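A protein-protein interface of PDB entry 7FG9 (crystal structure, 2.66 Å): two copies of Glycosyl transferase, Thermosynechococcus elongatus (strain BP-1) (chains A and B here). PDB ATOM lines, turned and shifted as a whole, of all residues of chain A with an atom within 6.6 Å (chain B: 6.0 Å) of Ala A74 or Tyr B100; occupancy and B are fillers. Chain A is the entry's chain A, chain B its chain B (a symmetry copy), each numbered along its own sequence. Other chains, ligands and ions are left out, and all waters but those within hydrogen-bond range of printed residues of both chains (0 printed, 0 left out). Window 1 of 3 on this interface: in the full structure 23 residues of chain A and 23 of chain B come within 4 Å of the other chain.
Of the 10 printed residues of chain B, 4 touch a printed residue of chain A. Printed residues of chain A that touch a printed residue of chain B: Glu A72, Ala A74, Val A75, Ala A78 and Leu A79. Hydrophobic or aromatic side chains of chain A that line the printed part of chain B: Ala A74, Val A75, Ala A78 and Leu A79. Among the printed residues, no Asp or Glu carboxylate lies within 4 Å of a Lys or Arg side-chain nitrogen of the other chain.
Trp A13 touches none of the printed residues of chain B. Printed residues of chain B within 4 Å of Glu A72: Asn B125. Of the printed residues of chain B, Ala A74 touches Tyr B100 (3.3 Å). Of the printed residues of chain B, Ala A78 touches Pro B104 and Ile B128. Of the printed residues of chain B, Leu A79 touches Ile B128. Tyr B100 touches two residues of chain A. The nearest residue of chain A that does not touch Tyr B100 is Glu A72 (4.2 Å).
No position is printed for both chains.
Among the printed residues, pairs that only touch across the chains: Ala A74 with Tyr B100, Val A75 with Tyr B100, Ala A78 with Pro B104, Ala A78 with Ile B128, Leu A79 with Ile B128, Glu A72 with Asn B125, Val A75 with Ile B128 and Val A75 with Asn B125.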
ATOM      1  N   TRP A  13      -4.861   3.848  14.983  1.00  0.00           N
ATOM      2  CA  TRP A  13      -4.930   3.834  16.448  1.00  0.00           C
ATOM      3  C   TRP A  13      -4.321   2.560  17.016  1.00  0.00           C
ATOM      4  O   TRP A  13      -3.677   2.592  18.070  1.00  0.00           O
ATOM      5  CB  TRP A  13      -6.377   3.966  16.941  1.00  0.00           C
ATOM      6  CG  TRP A  13      -7.070   5.261  16.647  1.00  0.00           C
ATOM      7  CD1 TRP A  13      -8.051   5.474  15.711  1.00  0.00           C
ATOM      8  CD2 TRP A  13      -6.869   6.525  17.306  1.00  0.00           C
ATOM      9  NE1 TRP A  13      -8.465   6.793  15.739  1.00  0.00           N
ATOM     10  CE2 TRP A  13      -7.756   7.460  16.703  1.00  0.00           C
ATOM     11  CE3 TRP A  13      -6.028   6.961  18.349  1.00  0.00           C
ATOM     12  CZ2 TRP A  13      -7.826   8.794  17.106  1.00  0.00           C
ATOM     13  CZ3 TRP A  13      -6.101   8.294  18.757  1.00  0.00           C
ATOM     14  CH2 TRP A  13      -6.991   9.197  18.128  1.00  0.00           C
ATOM     15  N   GLN A  71      -0.085  13.099  19.981  1.00  0.00           N
ATOM     16  CA  GLN A  71      -1.279  13.751  20.512  1.00  0.00           C
ATOM     17  C   GLN A  71      -2.109  14.436  19.430  1.00  0.00           C
ATOM     18  O   GLN A  71      -2.994  15.241  19.765  1.00  0.00           O
ATOM     19  CB  GLN A  71      -0.900  14.775  21.594  1.00  0.00           C
ATOM     20  CG  GLN A  71      -0.094  14.202  22.762  1.00  0.00           C
ATOM     21  CD  GLN A  71       0.897  15.196  23.328  1.00  0.00           C
ATOM     22  OE1 GLN A  71       0.751  16.409  23.143  1.00  0.00           O
ATOM     23  NE2 GLN A  71       1.913  14.689  24.031  1.00  0.00           N
ATOM     24  N   GLU A  72      -1.850  14.139  18.156  1.00  0.00           N
ATOM     25  CA  GLU A  72      -2.482  14.749  16.980  1.00  0.00           C
ATOM     26  C   GLU A  72      -2.691  13.700  15.900  1.00  0.00           C
ATOM     27  O   GLU A  72      -1.995  13.666  14.875  1.00  0.00           O
ATOM     28  CB  GLU A  72      -1.679  15.959  16.477  1.00  0.00           C
ATOM     29  CG  GLU A  72      -2.151  17.306  17.016  1.00  0.00           C
ATOM     30  CD  GLU A  72      -1.194  18.458  16.713  1.00  0.00           C
ATOM     31  OE1 GLU A  72       0.029  18.261  16.624  1.00  0.00           O
ATOM     32  OE2 GLU A  72      -1.699  19.527  16.313  1.00  0.00           O
ATOM     33  N   TYR A  73      -3.706  12.867  16.119  1.00  0.00           N
ATOM     34  CA  TYR A  73      -4.002  11.786  15.191  1.00  0.00           C
ATOM     35  C   TYR A  73      -4.168  12.299  13.769  1.00  0.00           C
ATOM     36  O   TYR A  73      -3.645  11.694  12.824  1.00  0.00           O
ATOM     37  CB  TYR A  73      -5.260  11.047  15.645  1.00  0.00           C
ATOM     38  CG  TYR A  73      -5.626   9.878  14.770  1.00  0.00           C
ATOM     39  CD1 TYR A  73      -5.117   8.612  15.030  1.00  0.00           C
ATOM     40  CD2 TYR A  73      -6.478  10.034  13.689  1.00  0.00           C
ATOM     41  CE1 TYR A  73      -5.445   7.538  14.238  1.00  0.00           C
ATOM     42  CE2 TYR A  73      -6.808   8.971  12.889  1.00  0.00           C
ATOM     43  CZ  TYR A  73      -6.293   7.719  13.167  1.00  0.00           C
ATOM     44  OH  TYR A  73      -6.621   6.634  12.371  1.00  0.00           O
ATOM     45  N   ALA A  74      -4.863  13.430  13.600  1.00  0.00           N
ATOM     46  CA  ALA A  74      -5.106  13.980  12.263  1.00  0.00           C
ATOM     47  C   ALA A  74      -3.816  14.190  11.468  1.00  0.00           C
ATOM     48  O   ALA A  74      -3.814  14.020  10.244  1.00  0.00           O
ATOM     49  CB  ALA A  74      -5.882  15.297  12.362  1.00  0.00           C
ATOM     50  N   VAL A  75      -2.720  14.573  12.131  1.00  0.00           N
ATOM     51  CA  VAL A  75      -1.446  14.710  11.429  1.00  0.00           C
ATOM     52  C   VAL A  75      -1.108  13.412  10.704  1.00  0.00           C
ATOM     53  O   VAL A  75      -0.867  13.393   9.487  1.00  0.00           O
ATOM     54  CB  VAL A  75      -0.329  15.105  12.416  1.00  0.00           C
ATOM     55  CG1 VAL A  75       1.042  14.993  11.758  1.00  0.00           C
ATOM     56  CG2 VAL A  75      -0.556  16.507  12.961  1.00  0.00           C
ATOM     57  N   TYR A  76      -1.122  12.299  11.442  1.00  0.00           N
ATOM     58  CA  TYR A  76      -0.725  11.020  10.874  1.00  0.00           C
ATOM     59  C   TYR A  76      -1.778  10.492   9.919  1.00  0.00           C
ATOM     60  O   TYR A  76      -1.435   9.849   8.914  1.00  0.00           O
ATOM     61  CB  TYR A  76      -0.423  10.024  12.000  1.00  0.00           C
ATOM     62  CG  TYR A  76       0.674  10.559  12.879  1.00  0.00           C
ATOM     63  CD1 TYR A  76       1.988  10.540  12.444  1.00  0.00           C
ATOM     64  CD2 TYR A  76       0.392  11.149  14.116  1.00  0.00           C
ATOM     65  CE1 TYR A  76       3.003  11.060  13.219  1.00  0.00           C
ATOM     66  CE2 TYR A  76       1.402  11.674  14.905  1.00  0.00           C
ATOM     67  CZ  TYR A  76       2.712  11.624  14.445  1.00  0.00           C
ATOM     68  OH  TYR A  76       3.746  12.138  15.187  1.00  0.00           O
ATOM     69  N   GLU A  77      -3.054  10.780  10.198  1.00  0.00           N
ATOM     70  CA  GLU A  77      -4.111  10.464   9.246  1.00  0.00           C
ATOM     71  C   GLU A  77      -3.895  11.191   7.927  1.00  0.00           C
ATOM     72  O   GLU A  77      -3.910  10.573   6.858  1.00  0.00           O
ATOM     73  CB  GLU A  77      -5.472  10.823   9.824  1.00  0.00           C
ATOM     74  CG  GLU A  77      -6.611  10.381   8.929  1.00  0.00           C
ATOM     75  CD  GLU A  77      -7.954  10.610   9.579  1.00  0.00           C
ATOM     76  OE1 GLU A  77      -8.281  11.797   9.826  1.00  0.00           O
ATOM     77  OE2 GLU A  77      -8.667   9.607   9.847  1.00  0.00           O
ATOM     78  N   ALA A  78      -3.682  12.512   7.986  1.00  0.00           N
ATOM     79  CA  ALA A  78      -3.454  13.281   6.769  1.00  0.00           C
ATOM     80  C   ALA A  78      -2.198  12.818   6.044  1.00  0.00           C
ATOM     81  O   ALA A  78      -2.155  12.843   4.805  1.00  0.00           O
ATOM     82  CB  ALA A  78      -3.363  14.769   7.090  1.00  0.00           C
ATOM     83  N   LEU A  79      -1.166  12.398   6.789  1.00  0.00           N
ATOM     84  CA  LEU A  79       0.024  11.859   6.140  1.00  0.00           C
ATOM     85  C   LEU A  79      -0.306  10.585   5.382  1.00  0.00           C
ATOM     86  O   LEU A  79       0.137  10.392   4.244  1.00  0.00           O
ATOM     87  CB  LEU A  79       1.110  11.574   7.171  1.00  0.00           C
ATOM     88  CG  LEU A  79       2.153  12.638   7.470  1.00  0.00           C
ATOM     89  CD1 LEU A  79       2.853  12.313   8.775  1.00  0.00           C
ATOM     90  CD2 LEU A  79       3.140  12.734   6.335  1.00  0.00           C
ATOM     91  N   VAL B  98      -6.266  26.823   6.772  1.00  0.00           N
ATOM     92  CA  VAL B  98      -6.775  25.729   7.605  1.00  0.00           C
ATOM     93  C   VAL B  98      -5.679  24.812   8.153  1.00  0.00           C
ATOM     94  O   VAL B  98      -5.999  23.841   8.845  1.00  0.00           O
ATOM     95  CB  VAL B  98      -7.830  24.878   6.852  1.00  0.00           C
ATOM     96  CG1 VAL B  98      -8.991  25.743   6.379  1.00  0.00           C
ATOM     97  CG2 VAL B  98      -7.199  24.081   5.683  1.00  0.00           C
ATOM     98  N   GLY B  99      -4.414  25.078   7.876  1.00  0.00           N
ATOM     99  CA  GLY B  99      -3.353  24.264   8.453  1.00  0.00           C
ATOM    100  C   GLY B  99      -3.056  23.009   7.652  1.00  0.00           C
ATOM    101  O   GLY B  99      -3.440  22.867   6.490  1.00  0.00           O
ATOM    102  N   TYR B 100      -2.414  22.049   8.331  1.00  0.00           N
ATOM    103  CA  TYR B 100      -1.720  20.948   7.665  1.00  0.00           C
ATOM    104  C   TYR B 100      -2.636  19.996   6.910  1.00  0.00           C
ATOM    105  O   TYR B 100      -2.141  19.259   6.056  1.00  0.00           O
ATOM    106  CB  TYR B 100      -0.891  20.140   8.669  1.00  0.00           C
ATOM    107  CG  TYR B 100      -1.676  19.536   9.815  1.00  0.00           C
ATOM    108  CD1 TYR B 100      -2.509  18.429   9.615  1.00  0.00           C
ATOM    109  CD2 TYR B 100      -1.567  20.046  11.102  1.00  0.00           C
ATOM    110  CE1 TYR B 100      -3.235  17.870  10.672  1.00  0.00           C
ATOM    111  CE2 TYR B 100      -2.272  19.502  12.152  1.00  0.00           C
ATOM    112  CZ  TYR B 100      -3.109  18.411  11.939  1.00  0.00           C
ATOM    113  OH  TYR B 100      -3.822  17.854  12.990  1.00  0.00           O
ATOM    114  N   THR B 101      -3.946  19.969   7.194  1.00  0.00           N
ATOM    115  CA  THR B 101      -4.790  19.033   6.448  1.00  0.00           C
ATOM    116  C   THR B 101      -4.833  19.382   4.964  1.00  0.00           C
ATOM    117  O   THR B 101      -5.120  18.512   4.134  1.00  0.00           O
ATOM    118  CB  THR B 101      -6.232  18.972   7.002  1.00  0.00           C
ATOM    119  OG1 THR B 101      -6.815  20.281   7.073  1.00  0.00           O
ATOM    120  CG2 THR B 101      -6.252  18.328   8.388  1.00  0.00           C
ATOM    121  N   ALA B 102      -4.546  20.631   4.609  1.00  0.00           N
ATOM    122  CA  ALA B 102      -4.544  21.010   3.209  1.00  0.00           C
ATOM    123  C   ALA B 102      -3.289  20.551   2.479  1.00  0.00           C
ATOM    124  O   ALA B 102      -3.271  20.578   1.244  1.00  0.00           O
ATOM    125  CB  ALA B 102      -4.697  22.521   3.080  1.00  0.00           C
ATOM    126  N   LEU B 103      -2.249  20.119   3.196  1.00  0.00           N
ATOM    127  CA  LEU B 103      -1.001  19.763   2.525  1.00  0.00           C
ATOM    128  C   LEU B 103      -1.135  18.616   1.527  1.00  0.00           C
ATOM    129  O   LEU B 103      -0.636  18.759   0.397  1.00  0.00           O
ATOM    130  CB  LEU B 103       0.079  19.465   3.563  1.00  0.00           C
ATOM    131  CG  LEU B 103       0.419  20.652   4.456  1.00  0.00           C
ATOM    132  CD1 LEU B 103       1.523  20.259   5.456  1.00  0.00           C
ATOM    133  CD2 LEU B 103       0.824  21.854   3.615  1.00  0.00           C
ATOM    134  N   PRO B 104      -1.743  17.468   1.854  1.00  0.00           N
ATOM    135  CA  PRO B 104      -1.697  16.353   0.887  1.00  0.00           C
ATOM    136  C   PRO B 104      -2.567  16.576  -0.334  1.00  0.00           C
ATOM    137  O   PRO B 104      -2.195  16.128  -1.428  1.00  0.00           O
ATOM    138  CB  PRO B 104      -2.146  15.131   1.702  1.00  0.00           C
ATOM    139  CG  PRO B 104      -2.710  15.656   2.957  1.00  0.00           C
ATOM    140  CD  PRO B 104      -2.264  17.054   3.167  1.00  0.00           C
ATOM    141  N   ASN B 125       3.163  17.923  14.472  1.00  0.00           N
ATOM    142  CA  ASN B 125       2.875  18.509  13.160  1.00  0.00           C
ATOM    143  C   ASN B 125       4.128  18.835  12.357  1.00  0.00           C
ATOM    144  O   ASN B 125       4.012  19.062  11.143  1.00  0.00           O
ATOM    145  CB  ASN B 125       1.951  19.746  13.281  1.00  0.00           C
ATOM    146  CG  ASN B 125       2.640  21.015  13.849  1.00  0.00           C
ATOM    147  OD1 ASN B 125       3.833  21.255  13.674  1.00  0.00           O
ATOM    148  ND2 ASN B 125       1.845  21.847  14.512  1.00  0.00           N
ATOM    149  N   ILE B 128       4.445  16.216   9.498  1.00  0.00           N
ATOM    150  CA  ILE B 128       3.774  16.374   8.200  1.00  0.00           C
ATOM    151  C   ILE B 128       4.307  17.583   7.439  1.00  0.00           C
ATOM    152  O   ILE B 128       4.371  17.561   6.201  1.00  0.00           O
ATOM    153  CB  ILE B 128       2.235  16.444   8.350  1.00  0.00           C
ATOM    154  CG1 ILE B 128       1.542  16.373   6.990  1.00  0.00           C
ATOM    155  CG2 ILE B 128       1.830  17.677   9.134  1.00  0.00           C
ATOM    156  CD1 ILE B 128       0.031  16.292   7.101  1.00  0.00           C
ATOM    157  N   PHE B 129       4.677  18.663   8.148  1.00  0.00           N
ATOM    158  CA  PHE B 129       5.209  19.847   7.468  1.00  0.00           C
ATOM    159  C   PHE B 129       6.532  19.536   6.789  1.00  0.00           C
ATOM    160  O   PHE B 129       6.749  19.907   5.626  1.00  0.00           O
ATOM    161  CB  PHE B 129       5.368  21.012   8.448  1.00  0.00           C
ATOM    162  CG  PHE B 129       4.080  21.741   8.713  1.00  0.00           C
ATOM    163  CD1 PHE B 129       3.415  22.376   7.674  1.00  0.00           C
ATOM    164  CD2 PHE B 129       3.517  21.762   9.995  1.00  0.00           C
ATOM    165  CE1 PHE B 129       2.206  23.020   7.913  1.00  0.00           C
ATOM    166  CE2 PHE B 129       2.321  22.402  10.241  1.00  0.00           C
ATOM    167  CZ  PHE B 129       1.658  23.036   9.205  1.00  0.00           C
